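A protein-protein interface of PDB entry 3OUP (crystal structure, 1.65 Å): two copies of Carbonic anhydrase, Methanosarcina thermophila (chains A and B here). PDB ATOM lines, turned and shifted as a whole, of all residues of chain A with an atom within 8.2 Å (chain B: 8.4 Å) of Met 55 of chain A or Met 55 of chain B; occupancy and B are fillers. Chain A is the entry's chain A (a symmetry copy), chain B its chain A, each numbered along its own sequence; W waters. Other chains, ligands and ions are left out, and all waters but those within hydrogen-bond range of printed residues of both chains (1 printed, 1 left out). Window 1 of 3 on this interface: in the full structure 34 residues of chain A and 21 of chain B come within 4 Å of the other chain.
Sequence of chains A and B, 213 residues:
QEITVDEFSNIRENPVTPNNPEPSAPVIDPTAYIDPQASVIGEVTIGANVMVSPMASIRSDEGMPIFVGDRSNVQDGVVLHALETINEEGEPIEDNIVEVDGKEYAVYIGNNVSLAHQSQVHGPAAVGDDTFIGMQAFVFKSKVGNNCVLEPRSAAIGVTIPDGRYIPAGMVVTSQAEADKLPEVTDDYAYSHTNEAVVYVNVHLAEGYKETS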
ATOM      1  N   ASN A  10      18.404  18.491   2.467  1.00  0.00           N
ATOM      2  CA  ASN A  10      18.167  17.695   1.263  1.00  0.00           C
ATOM      3  C   ASN A  10      18.140  18.513  -0.035  1.00  0.00           C
ATOM      4  O   ASN A  10      18.031  17.943  -1.118  1.00  0.00           O
ATOM      5  CB  ASN A  10      16.849  16.954   1.391  1.00  0.00           C
ATOM      6  CG  ASN A  10      15.673  17.892   1.442  1.00  0.00           C
ATOM      7  OD1 ASN A  10      15.705  18.944   2.111  1.00  0.00           O
ATOM      8  ND2 ASN A  10      14.629  17.536   0.740  1.00  0.00           N
ATOM      9  N   ASP A  35       9.548  17.043  -1.037  1.00  0.00           N
ATOM     10  CA  ASP A  35       9.439  16.192   0.141  1.00  0.00           C
ATOM     11  C   ASP A  35      10.764  16.155   0.878  1.00  0.00           C
ATOM     12  O   ASP A  35      11.829  16.159   0.265  1.00  0.00           O
ATOM     13  CB  ASP A  35       9.051  14.770  -0.279  1.00  0.00           C
ATOM     14  CG  ASP A  35       8.616  13.934   0.903  1.00  0.00           C
ATOM     15  OD1 ASP A  35       7.427  14.055   1.272  1.00  0.00           O
ATOM     16  OD2 ASP A  35       9.449  13.210   1.469  1.00  0.00           O
ATOM     17  N   PRO A  36      10.721  16.121   2.202  1.00  0.00           N
ATOM     18  CA  PRO A  36      11.965  16.032   2.968  1.00  0.00           C
ATOM     19  C   PRO A  36      12.791  14.804   2.650  1.00  0.00           C
ATOM     20  O   PRO A  36      13.999  14.819   2.912  1.00  0.00           O
ATOM     21  CB  PRO A  36      11.470  15.927   4.425  1.00  0.00           C
ATOM     22  CG  PRO A  36      10.122  16.522   4.418  1.00  0.00           C
ATOM     23  CD  PRO A  36       9.524  16.280   3.055  1.00  0.00           C
ATOM     24  N   GLN A  37      12.165  13.745   2.114  1.00  0.00           N
ATOM     25  CA  GLN A  37      12.929  12.555   1.764  1.00  0.00           C
ATOM     26  C   GLN A  37      13.248  12.459   0.263  1.00  0.00           C
ATOM     27  O   GLN A  37      13.668  11.398  -0.229  1.00  0.00           O
ATOM     28  CB  GLN A  37      12.188  11.288   2.236  1.00  0.00           C
ATOM     29  CG  GLN A  37      12.302  11.168   3.779  1.00  0.00           C
ATOM     30  CD  GLN A  37      11.537   9.993   4.375  1.00  0.00           C
ATOM     31  OE1 GLN A  37      10.340  10.069   4.581  1.00  0.00           O
ATOM     32  NE2 GLN A  37      12.242   8.937   4.694  1.00  0.00           N
ATOM     33  N   ALA A  38      13.128  13.579  -0.437  1.00  0.00           N
ATOM     34  CA  ALA A  38      13.686  13.691  -1.792  1.00  0.00           C
ATOM     35  C   ALA A  38      15.037  14.357  -1.696  1.00  0.00           C
ATOM     36  O   ALA A  38      15.392  14.913  -0.640  1.00  0.00           O
ATOM     37  CB  ALA A  38      12.762  14.525  -2.674  1.00  0.00           C
ATOM     38  N   SER A  39      15.822  14.265  -2.772  1.00  0.00           N
ATOM     39  CA  SER A  39      17.133  14.930  -2.824  1.00  0.00           C
ATOM     40  C   SER A  39      17.159  15.806  -4.081  1.00  0.00           C
ATOM     41  O   SER A  39      16.830  15.329  -5.149  1.00  0.00           O
ATOM     42  CB  SER A  39      18.236  13.863  -2.957  1.00  0.00           C
ATOM     43  OG  SER A  39      19.504  14.496  -3.056  1.00  0.00           O
ATOM     44  N   VAL A  40      17.567  17.076  -3.947  1.00  0.00           N
ATOM     45  CA  VAL A  40      17.676  17.952  -5.102  1.00  0.00           C
ATOM     46  C   VAL A  40      19.034  18.641  -4.976  1.00  0.00           C
ATOM     47  O   VAL A  40      19.286  19.376  -4.000  1.00  0.00           O
ATOM     48  CB  VAL A  40      16.595  19.043  -5.092  1.00  0.00           C
ATOM     49  CG1 VAL A  40      16.723  19.884  -6.343  1.00  0.00           C
ATOM     50  CG2 VAL A  40      15.175  18.400  -5.031  1.00  0.00           C
ATOM     51  N   VAL A  52       7.470  17.115  -5.720  1.00  0.00           N
ATOM     52  CA  VAL A  52       8.603  16.185  -5.777  1.00  0.00           C
ATOM     53  C   VAL A  52       8.431  15.232  -4.587  1.00  0.00           C
ATOM     54  O   VAL A  52       8.418  15.674  -3.421  1.00  0.00           O
ATOM     55  CB  VAL A  52       9.945  16.919  -5.718  1.00  0.00           C
ATOM     56  CG1 VAL A  52      11.115  15.890  -5.736  1.00  0.00           C
ATOM     57  CG2 VAL A  52      10.091  17.872  -6.895  1.00  0.00           C
ATOM     58  N   SER A  53       8.224  13.943  -4.894  1.00  0.00           N
ATOM     59  CA  SER A  53       7.833  12.935  -3.894  1.00  0.00           C
ATOM     60  C   SER A  53       9.014  12.291  -3.198  1.00  0.00           C
ATOM     61  O   SER A  53      10.166  12.481  -3.581  1.00  0.00           O
ATOM     62  CB  SER A  53       7.088  11.809  -4.618  1.00  0.00           C
ATOM     63  OG  SER A  53       5.868  12.286  -5.122  1.00  0.00           O
ATOM     64  N   PRO A  54       8.736  11.532  -2.135  1.00  0.00           N
ATOM     65  CA  PRO A  54       9.793  10.805  -1.413  1.00  0.00           C
ATOM     66  C   PRO A  54      10.650   9.957  -2.331  1.00  0.00           C
ATOM     67  O   PRO A  54      10.178   9.318  -3.270  1.00  0.00           O
ATOM     68  CB  PRO A  54       8.994   9.887  -0.473  1.00  0.00           C
ATOM     69  CG  PRO A  54       7.697  10.636  -0.201  1.00  0.00           C
ATOM     70  CD  PRO A  54       7.396  11.289  -1.550  1.00  0.00           C
ATOM     71  N   MET A  55      11.942   9.944  -2.015  1.00  0.00           N
ATOM     72  CA  MET A  55      12.941   9.083  -2.641  1.00  0.00           C
ATOM     73  C   MET A  55      13.292   9.502  -4.079  1.00  0.00           C
ATOM     74  O   MET A  55      14.096   8.806  -4.739  1.00  0.00           O
ATOM     75  CB  MET A  55      12.520   7.610  -2.628  1.00  0.00           C
ATOM     76  CG  MET A  55      11.983   7.111  -1.309  1.00  0.00           C
ATOM     77  SD  MET A  55      13.115   7.437   0.047  1.00  0.00           S
ATOM     78  CE  MET A  55      12.003   6.960   1.403  1.00  0.00           C
ATOM     79  N   ALA A  56      12.751  10.627  -4.582  1.00  0.00           N
ATOM     80  CA  ALA A  56      13.201  11.101  -5.900  1.00  0.00           C
ATOM     81  C   ALA A  56      14.580  11.704  -5.744  1.00  0.00           C
ATOM     82  O   ALA A  56      14.889  12.265  -4.702  1.00  0.00           O
ATOM     83  CB  ALA A  56      12.229  12.139  -6.445  1.00  0.00           C
ATOM     84  N   SER A  57      15.400  11.577  -6.780  1.00  0.00           N
ATOM     85  CA  SER A  57      16.724  12.185  -6.746  1.00  0.00           C
ATOM     86  C   SER A  57      16.873  12.999  -7.997  1.00  0.00           C
ATOM     87  O   SER A  57      16.899  12.433  -9.081  1.00  0.00           O
ATOM     88  CB  SER A  57      17.796  11.111  -6.679  1.00  0.00           C
ATOM     89  OG  SER A  57      19.078  11.731  -6.585  1.00  0.00           O
ATOM     90  N   ILE A  58      17.025  14.320  -7.841  1.00  0.00           N
ATOM     91  CA  ILE A  58      17.264  15.206  -8.964  1.00  0.00           C
ATOM     92  C   ILE A  58      18.678  15.741  -8.743  1.00  0.00           C
ATOM     93  O   ILE A  58      18.895  16.433  -7.776  1.00  0.00           O
ATOM     94  CB  ILE A  58      16.245  16.325  -8.987  1.00  0.00           C
ATOM     95  CG1 ILE A  58      14.830  15.736  -9.085  1.00  0.00           C
ATOM     96  CG2 ILE A  58      16.542  17.240 -10.183  1.00  0.00           C
ATOM     97  CD1 ILE A  58      13.731  16.866  -8.957  1.00  0.00           C
ATOM     98  N   VAL A  74       7.232  14.955 -10.015  1.00  0.00           N
ATOM     99  CA  VAL A  74       8.385  14.042 -10.038  1.00  0.00           C
ATOM    100  C   VAL A  74       8.106  13.048  -8.918  1.00  0.00           C
ATOM    101  O   VAL A  74       8.206  13.375  -7.733  1.00  0.00           O
ATOM    102  CB  VAL A  74       9.678  14.809  -9.739  1.00  0.00           C
ATOM    103  CG1 VAL A  74      10.886  13.835  -9.749  1.00  0.00           C
ATOM    104  CG2 VAL A  74       9.889  15.938 -10.767  1.00  0.00           C
ATOM    105  N   GLN A  75       7.674  11.847  -9.290  1.00  0.00           N
ATOM    106  CA  GLN A  75       7.112  10.943  -8.305  1.00  0.00           C
ATOM    107  C   GLN A  75       8.163  10.068  -7.617  1.00  0.00           C
ATOM    108  O   GLN A  75       9.379  10.245  -7.812  1.00  0.00           O
ATOM    109  CB  GLN A  75       6.043  10.073  -8.956  1.00  0.00           C
ATOM    110  CG  GLN A  75       4.810  10.950  -9.424  1.00  0.00           C
ATOM    111  CD  GLN A  75       3.772  10.147 -10.146  1.00  0.00           C
ATOM    112  OE1 GLN A  75       3.681   8.927  -9.989  1.00  0.00           O
ATOM    113  NE2 GLN A  75       2.988  10.816 -10.982  1.00  0.00           N
ATOM    114  N   ASP A  76       7.671   9.155  -6.777  1.00  0.00           N
ATOM    115  CA  ASP A  76       8.572   8.487  -5.816  1.00  0.00           C
ATOM    116  C   ASP A  76       9.646   7.697  -6.562  1.00  0.00           C
ATOM    117  O   ASP A  76       9.333   6.968  -7.498  1.00  0.00           O
ATOM    118  CB  ASP A  76       7.827   7.475  -4.919  1.00  0.00           C
ATOM    119  CG  ASP A  76       6.485   8.012  -4.401  1.00  0.00           C
ATOM    120  OD1 ASP A  76       5.649   8.296  -5.257  1.00  0.00           O
ATOM    121  OD2 ASP A  76       6.292   8.090  -3.185  1.00  0.00           O
ATOM    122  N   GLY A  77      10.906   7.842  -6.143  1.00  0.00           N
ATOM    123  CA  GLY A  77      11.944   6.998  -6.740  1.00  0.00           C
ATOM    124  C   GLY A  77      12.390   7.431  -8.136  1.00  0.00           C
ATOM    125  O   GLY A  77      13.208   6.719  -8.736  1.00  0.00           O
ATOM    126  N   VAL A  78      11.895   8.559  -8.672  1.00  0.00           N
ATOM    127  CA  VAL A  78      12.304   9.004  -9.994  1.00  0.00           C
ATOM    128  C   VAL A  78      13.730   9.542  -9.900  1.00  0.00           C
ATOM    129  O   VAL A  78      14.084  10.153  -8.884  1.00  0.00           O
ATOM    130  CB  VAL A  78      11.361  10.101 -10.473  1.00  0.00           C
ATOM    131  CG1 VAL A  78      11.934  10.843 -11.737  1.00  0.00           C
ATOM    132  CG2 VAL A  78      10.033   9.437 -10.826  1.00  0.00           C
ATOM    133  N   VAL A  79      14.538   9.282 -10.924  1.00  0.00           N
ATOM    134  CA  VAL A  79      15.887   9.859 -10.959  1.00  0.00           C
ATOM    135  C   VAL A  79      16.025  10.761 -12.186  1.00  0.00           C
ATOM    136  O   VAL A  79      15.639  10.358 -13.300  1.00  0.00           O
ATOM    137  CB  VAL A  79      16.950   8.740 -11.030  1.00  0.00           C
ATOM    138  CG1 VAL A  79      18.393   9.345 -11.233  1.00  0.00           C
ATOM    139  CG2 VAL A  79      16.936   7.924  -9.737  1.00  0.00           C
ATOM    140  N   GLN A 118       9.265   5.690 -10.093  1.00  0.00           N
ATOM    141  CA  GLN A 118      10.408   4.839 -10.492  1.00  0.00           C
ATOM    142  C   GLN A 118      10.842   5.040 -11.952  1.00  0.00           C
ATOM    143  O   GLN A 118      11.697   4.283 -12.433  1.00  0.00           O
ATOM    144  CB  GLN A 118      10.155   3.329 -10.222  1.00  0.00           C
ATOM    145  CG  GLN A 118       9.960   3.018  -8.745  1.00  0.00           C
ATOM    146  CD  GLN A 118       9.690   1.555  -8.550  1.00  0.00           C
ATOM    147  OE1 GLN A 118       9.075   0.938  -9.409  1.00  0.00           O
ATOM    148  NE2 GLN A 118      10.062   1.009  -7.383  1.00  0.00           N
ATOM    149  N   ASP B  35      26.860   9.327   0.330  1.00  0.00           N
ATOM    150  CA  ASP B  35      25.896  10.411   0.473  1.00  0.00           C
ATOM    151  C   ASP B  35      25.079  10.214   1.735  1.00  0.00           C
ATOM    152  O   ASP B  35      24.742   9.090   2.102  1.00  0.00           O
ATOM    153  CB  ASP B  35      24.961  10.440  -0.740  1.00  0.00           C
ATOM    154  CG  ASP B  35      24.159  11.720  -0.800  1.00  0.00           C
ATOM    155  OD1 ASP B  35      24.718  12.711  -1.319  1.00  0.00           O
ATOM    156  OD2 ASP B  35      23.021  11.743  -0.308  1.00  0.00           O
ATOM    157  N   PRO B  36      24.748  11.298   2.421  1.00  0.00           N
ATOM    158  CA  PRO B  36      23.916  11.177   3.618  1.00  0.00           C
ATOM    159  C   PRO B  36      22.565  10.546   3.361  1.00  0.00           C
ATOM    160  O   PRO B  36      21.959  10.034   4.310  1.00  0.00           O
ATOM    161  CB  PRO B  36      23.700  12.644   4.042  1.00  0.00           C
ATOM    162  CG  PRO B  36      24.829  13.386   3.454  1.00  0.00           C
ATOM    163  CD  PRO B  36      25.226  12.677   2.183  1.00  0.00           C
ATOM    164  N   GLN B  37      22.076  10.590   2.112  1.00  0.00           N
ATOM    165  CA  GLN B  37      20.793   9.966   1.815  1.00  0.00           C
ATOM    166  C   GLN B  37      20.929   8.588   1.147  1.00  0.00           C
ATOM    167  O   GLN B  37      19.949   8.044   0.612  1.00  0.00           O
ATOM    168  CB  GLN B  37      19.935  10.903   0.940  1.00  0.00           C
ATOM    169  CG  GLN B  37      19.406  12.077   1.806  1.00  0.00           C
ATOM    170  CD  GLN B  37      18.608  13.118   1.031  1.00  0.00           C
ATOM    171  OE1 GLN B  37      19.172  13.988   0.394  1.00  0.00           O
ATOM    172  NE2 GLN B  37      17.305  13.051   1.133  1.00  0.00           N
ATOM    173  N   ALA B  38      22.111   7.997   1.254  1.00  0.00           N
ATOM    174  CA  ALA B  38      22.279   6.573   0.931  1.00  0.00           C
ATOM    175  C   ALA B  38      22.205   5.783   2.215  1.00  0.00           C
ATOM    176  O   ALA B  38      22.262   6.362   3.316  1.00  0.00           O
ATOM    177  CB  ALA B  38      23.630   6.342   0.260  1.00  0.00           C
ATOM    178  N   SER B  39      22.027   4.465   2.091  1.00  0.00           N
ATOM    179  CA  SER B  39      22.008   3.581   3.266  1.00  0.00           C
ATOM    180  C   SER B  39      23.049   2.481   3.037  1.00  0.00           C
ATOM    181  O   SER B  39      23.051   1.869   1.986  1.00  0.00           O
ATOM    182  CB  SER B  39      20.622   2.917   3.376  1.00  0.00           C
ATOM    183  OG  SER B  39      20.605   2.024   4.480  1.00  0.00           O
ATOM    184  N   VAL B  52      29.010   6.822  -3.589  1.00  0.00           N
ATOM    185  CA  VAL B  52      27.709   6.189  -3.348  1.00  0.00           C
ATOM    186  C   VAL B  52      26.685   7.329  -3.291  1.00  0.00           C
ATOM    187  O   VAL B  52      26.786   8.226  -2.431  1.00  0.00           O
ATOM    188  CB  VAL B  52      27.706   5.368  -2.056  1.00  0.00           C
ATOM    189  CG1 VAL B  52      26.295   4.752  -1.819  1.00  0.00           C
ATOM    190  CG2 VAL B  52      28.739   4.253  -2.123  1.00  0.00           C
ATOM    191  N   SER B  53      25.752   7.328  -4.255  1.00  0.00           N
ATOM    192  CA  SER B  53      24.827   8.452  -4.475  1.00  0.00           C
ATOM    193  C   SER B  53      23.566   8.365  -3.641  1.00  0.00           C
ATOM    194  O   SER B  53      23.293   7.355  -2.995  1.00  0.00           O
ATOM    195  CB  SER B  53      24.382   8.424  -5.940  1.00  0.00           C
ATOM    196  OG  SER B  53      25.472   8.704  -6.780  1.00  0.00           O
ATOM    197  N   PRO B  54      22.787   9.449  -3.624  1.00  0.00           N
ATOM    198  CA  PRO B  54      21.506   9.463  -2.900  1.00  0.00           C
ATOM    199  C   PRO B  54      20.610   8.299  -3.275  1.00  0.00           C
ATOM    200  O   PRO B  54      20.508   7.892  -4.430  1.00  0.00           O
ATOM    201  CB  PRO B  54      20.859  10.775  -3.377  1.00  0.00           C
ATOM    202  CG  PRO B  54      22.029  11.695  -3.699  1.00  0.00           C
ATOM    203  CD  PRO B  54      23.052  10.737  -4.309  1.00  0.00           C
ATOM    204  N   MET B  55      19.930   7.783  -2.255  1.00  0.00           N
ATOM    205  CA  MET B  55      18.888   6.769  -2.381  1.00  0.00           C
ATOM    206  C   MET B  55      19.434   5.374  -2.730  1.00  0.00           C
ATOM    207  O   MET B  55      18.630   4.434  -2.919  1.00  0.00           O
ATOM    208  CB  MET B  55      17.818   7.168  -3.403  1.00  0.00           C
ATOM    209  CG  MET B  55      17.318   8.587  -3.283  1.00  0.00           C
ATOM    210  SD  MET B  55      16.748   8.964  -1.622  1.00  0.00           S
ATOM    211  CE  MET B  55      16.522  10.752  -1.851  1.00  0.00           C
ATOM    212  N   ALA B  56      20.765   5.190  -2.789  1.00  0.00           N
ATOM    213  CA  ALA B  56      21.283   3.826  -2.979  1.00  0.00           C
ATOM    214  C   ALA B  56      21.128   3.073  -1.675  1.00  0.00           C
ATOM    215  O   ALA B  56      21.214   3.668  -0.610  1.00  0.00           O
ATOM    216  CB  ALA B  56      22.749   3.873  -3.390  1.00  0.00           C
ATOM    217  N   SER B  57      20.895   1.770  -1.771  1.00  0.00           N
ATOM    218  CA  SER B  57      20.799   0.952  -0.569  1.00  0.00           C
ATOM    219  C   SER B  57      21.730  -0.211  -0.746  1.00  0.00           C
ATOM    220  O   SER B  57      21.497  -1.038  -1.616  1.00  0.00           O
ATOM    221  CB  SER B  57      19.373   0.466  -0.374  1.00  0.00           C
ATOM    222  OG  SER B  57      19.293  -0.279   0.840  1.00  0.00           O
ATOM    223  N   ILE B  58      22.752  -0.301   0.114  1.00  0.00           N
ATOM    224  CA  ILE B  58      23.672  -1.421   0.104  1.00  0.00           C
ATOM    225  C   ILE B  58      23.427  -2.138   1.432  1.00  0.00           C
ATOM    226  O   ILE B  58      23.684  -1.560   2.462  1.00  0.00           O
ATOM    227  CB  ILE B  58      25.101  -0.938  -0.009  1.00  0.00           C
ATOM    228  CG1 ILE B  58      25.271  -0.117  -1.297  1.00  0.00           C
ATOM    229  CG2 ILE B  58      26.038  -2.154  -0.006  1.00  0.00           C
ATOM    230  CD1 ILE B  58      26.710   0.533  -1.374  1.00  0.00           C
ATOM    231  N   VAL B  74      28.313   3.739  -7.219  1.00  0.00           N
ATOM    232  CA  VAL B  74      27.010   3.119  -6.937  1.00  0.00           C
ATOM    233  C   VAL B  74      26.016   4.271  -7.011  1.00  0.00           C
ATOM    234  O   VAL B  74      25.963   5.126  -6.123  1.00  0.00           O
ATOM    235  CB  VAL B  74      27.000   2.516  -5.528  1.00  0.00           C
ATOM    236  CG1 VAL B  74      25.616   1.879  -5.234  1.00  0.00           C
ATOM    237  CG2 VAL B  74      28.118   1.464  -5.381  1.00  0.00           C
ATOM    238  N   GLN B  75      25.278   4.344  -8.114  1.00  0.00           N
ATOM    239  CA  GLN B  75      24.525   5.549  -8.402  1.00  0.00           C
ATOM    240  C   GLN B  75      23.128   5.553  -7.776  1.00  0.00           C
ATOM    241  O   GLN B  75      22.768   4.657  -6.991  1.00  0.00           O
ATOM    242  CB  GLN B  75      24.429   5.748  -9.910  1.00  0.00           C
ATOM    243  CG  GLN B  75      25.857   6.026 -10.534  1.00  0.00           C
ATOM    244  CD  GLN B  75      25.822   6.144 -12.027  1.00  0.00           C
ATOM    245  OE1 GLN B  75      24.783   6.437 -12.622  1.00  0.00           O
ATOM    246  NE2 GLN B  75      26.956   5.881 -12.664  1.00  0.00           N
ATOM    247  N   ASP B  76      22.369   6.603  -8.103  1.00  0.00           N
ATOM    248  CA  ASP B  76      21.151   6.894  -7.318  1.00  0.00           C
ATOM    249  C   ASP B  76      20.165   5.733  -7.426  1.00  0.00           C
ATOM    250  O   ASP B  76      19.912   5.241  -8.521  1.00  0.00           O
ATOM    251  CB  ASP B  76      20.411   8.148  -7.831  1.00  0.00           C
ATOM    252  CG  ASP B  76      21.360   9.311  -8.156  1.00  0.00           C
ATOM    253  OD1 ASP B  76      22.194   9.099  -9.035  1.00  0.00           O
ATOM    254  OD2 ASP B  76      21.221  10.388  -7.573  1.00  0.00           O
ATOM    255  N   GLY B  77      19.609   5.304  -6.289  1.00  0.00           N
ATOM    256  CA  GLY B  77      18.556   4.287  -6.365  1.00  0.00           C
ATOM    257  C   GLY B  77      19.060   2.868  -6.620  1.00  0.00           C
ATOM    258  O   GLY B  77      18.222   1.968  -6.776  1.00  0.00           O
ATOM    259  N   VAL B  78      20.381   2.630  -6.667  1.00  0.00           N
ATOM    260  CA  VAL B  78      20.895   1.290  -6.901  1.00  0.00           C
ATOM    261  C   VAL B  78      20.678   0.465  -5.633  1.00  0.00           C
ATOM    262  O   VAL B  78      20.792   1.008  -4.527  1.00  0.00           O
ATOM    263  CB  VAL B  78      22.381   1.367  -7.226  1.00  0.00           C
ATOM    264  CG1 VAL B  78      23.059  -0.051  -7.168  1.00  0.00           C
ATOM    265  CG2 VAL B  78      22.509   1.939  -8.636  1.00  0.00           C
ATOM    266  N   VAL B  79      20.333  -0.809  -5.799  1.00  0.00           N
ATOM    267  CA  VAL B  79      20.216  -1.694  -4.634  1.00  0.00           C
ATOM    268  C   VAL B  79      21.222  -2.840  -4.760  1.00  0.00           C
ATOM    269  O   VAL B  79      21.324  -3.460  -5.835  1.00  0.00           O
ATOM    270  CB  VAL B  79      18.789  -2.280  -4.544  1.00  0.00           C
ATOM    271  CG1 VAL B  79      18.693  -3.357  -3.395  1.00  0.00           C
ATOM    272  CG2 VAL B  79      17.784  -1.163  -4.256  1.00  0.00           C
ATOM    273  N   LEU B  80      21.974  -3.095  -3.685  1.00  0.00           N
ATOM    274  CA  LEU B  80      22.802  -4.302  -3.580  1.00  0.00           C
ATOM    275  C   LEU B  80      22.312  -5.075  -2.359  1.00  0.00           C
ATOM    276  O   LEU B  80      22.213  -4.513  -1.276  1.00  0.00           O
ATOM    277  CB  LEU B  80      24.287  -3.952  -3.376  1.00  0.00           C
ATOM    278  CG  LEU B  80      24.919  -3.094  -4.480  1.00  0.00           C
ATOM    279  CD1 LEU B  80      26.369  -2.794  -4.116  1.00  0.00           C
ATOM    280  CD2 LEU B  80      24.861  -3.852  -5.793  1.00  0.00           C
ATOM    281  N   GLN B 118      19.480   3.330 -10.650  1.00  0.00           N
ATOM    282  CA  GLN B 118      18.325   2.411 -10.551  1.00  0.00           C
ATOM    283  C   GLN B 118      18.651   0.969 -10.969  1.00  0.00           C
ATOM    284  O   GLN B 118      17.729   0.147 -11.056  1.00  0.00           O
ATOM    285  CB  GLN B 118      17.084   2.918 -11.339  1.00  0.00           C
ATOM    286  CG  GLN B 118      16.550   4.241 -10.811  1.00  0.00           C
ATOM    287  CD  GLN B 118      15.375   4.694 -11.628  1.00  0.00           C
ATOM    288  OE1 GLN B 118      15.338   4.432 -12.823  1.00  0.00           O
ATOM    289  NE2 GLN B 118      14.455   5.454 -11.018  1.00  0.00           N
ATOM    290  N   SER B 119      19.921   0.654 -11.234  1.00  0.00           N
ATOM    291  CA  SER B 119      20.264  -0.762 -11.465  1.00  0.00           C
ATOM    292  C   SER B 119      20.242  -1.549 -10.136  1.00  0.00           C
ATOM    293  O   SER B 119      20.090  -0.976  -9.044  1.00  0.00           O
ATOM    294  CB  SER B 119      21.636  -0.882 -12.158  1.00  0.00           C
ATOM    295  OG  SER B 119      22.694  -0.423 -11.298  1.00  0.00           O
HETATM  296  O   HOH W   1      15.404  10.303   1.635  1.00  0.00           O
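Ala 38 of chain A touches Gln 37 of chain B, but with the chains exchanged Gln 37 of chain A does not touch Ala 38 of chain B (9.2 Å).
Ala 56 of chain A touches Met 55 of chain B, but with the chains exchanged Met 55 of chain A does not touch Ala 56 of chain B (7.8 Å).
Gly 77 of chain A touches Gln 118 of chain B, but with the chains exchanged Gln 118 of chain A does not touch Gly 77 of chain B (8.2 Å).
Val 79 of chain A touches Asp 76 of chain B, but with the chains exchanged Asp 76 of chain A does not touch Val 79 of chain B (12.2 Å).
The backbone carbonyl oxygen of Pro 54 of chain B lies within hydrogen-bond range of the backbone NH of Gly 77 of chain B, at 3.3 Å.
O of Asp 35 of chain A is in hydrogen-bond range of ND2 of Asn 10 of chain A (3.2 Å).
O of Ala 38 of chain A lies within hydrogen-bond range of ND2 of Asn 10 of chain A.
The side-chain carboxylate of Asp 35 of chain A lies within hydrogen-bond range of the backbone NH of Gln 37 of chain A.
The backbone carbonyl oxygen (O) of Ala 56 of chain A is in hydrogen-bond range of the backbone NH (N) of Ser 39 of chain A (2.9 Å).
The backbone NH (N) of Ser 57 of chain A lies within hydrogen-bond range of the backbone carbonyl oxygen (O) of Val 78 of chain A, 2.9 Å away.
Of the printed residues of chain B, Asn 10 of chain A touches Gln 37 (3.9 Å).
Printed residues of chain B within 4 Å of Gln 37 of chain A: Met 55 (3.3 Å).
Met 55 of chain A touches just one residue of chain B: Met 55 (3.5 Å).
Of the printed residues of chain B, Ala 56 of chain A touches Met 55 (3.6 Å).
Of the printed residues of chain B, Gly 77 of chain A touches Gln 118.
Of the printed residues of chain B, Val 79 of chain A touches Asp 76 (3.97 Å) and Gln 118 (3.7 Å).
Of the printed residues of chain A, Gln 37 of chain B touches Asn 10, Ala 38 and Ser 39.
Met 55 of chain B touches five residues of chain A.
Ala 56 of chain B touches none of the printed residues of chain A.
Ile 58 of chain B touches none of the printed residues of chain A.
The nearest printed residue of chain A that does not touch Pro 54 of chain B is Ala 56 of chain A (6.3 Å).
Water W1 lies within hydrogen-bond range of the backbone carbonyl oxygen of Gln 37 of chain A, the side-chain amide nitrogen of Gln 37 of chain B and the side-chain sulfur of Met 55 of chain B.
Along chain A the printed residues that touch a printed residue of chain B span positions 10 to 118.
Among the printed residues, pairs that only touch across the chains: Asn 10 of chain A with Gln 37 of chain B, Gln 37 of chain A with Met 55 of chain B, Ala 38 of chain A with Met 55 of chain B, Ser 39 of chain A with Gln 37 of chain B, Ser 39 of chain A with Pro 54 of chain B, Ser 39 of chain A with Met 55 of chain B, Met 55 of chain A with Met 55 of chain B, Ala 56 of chain A with Met 55 of chain B, Ser 57 of chain A with Pro 54 of chain B, Val 79 of chain A with Asp 76 of chain B and Val 79 of chain A with Gln 118 of chain B.
The side-chain amide nitrogen (NE2) of Gln 37 of chain B is in hydrogen-bond range of the backbone carbonyl oxygen (O) of Ala 38 of chain A (3.2 Å).
The side-chain hydroxyl (OG) of Ser 57 of chain A is in hydrogen-bond range of the side-chain carboxylate (OD2) of Asp 76 of chain B.
The side-chain amide nitrogen (NE2) of Gln 118 of chain B sits at hydrogen-bond distance from the backbone carbonyl oxygen (O) of Gly 77 of chain A (2.9 Å).
O of Gln 118 of chain A is in hydrogen-bond range of NE2 of Gln 118 of chain B (3.3 Å).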
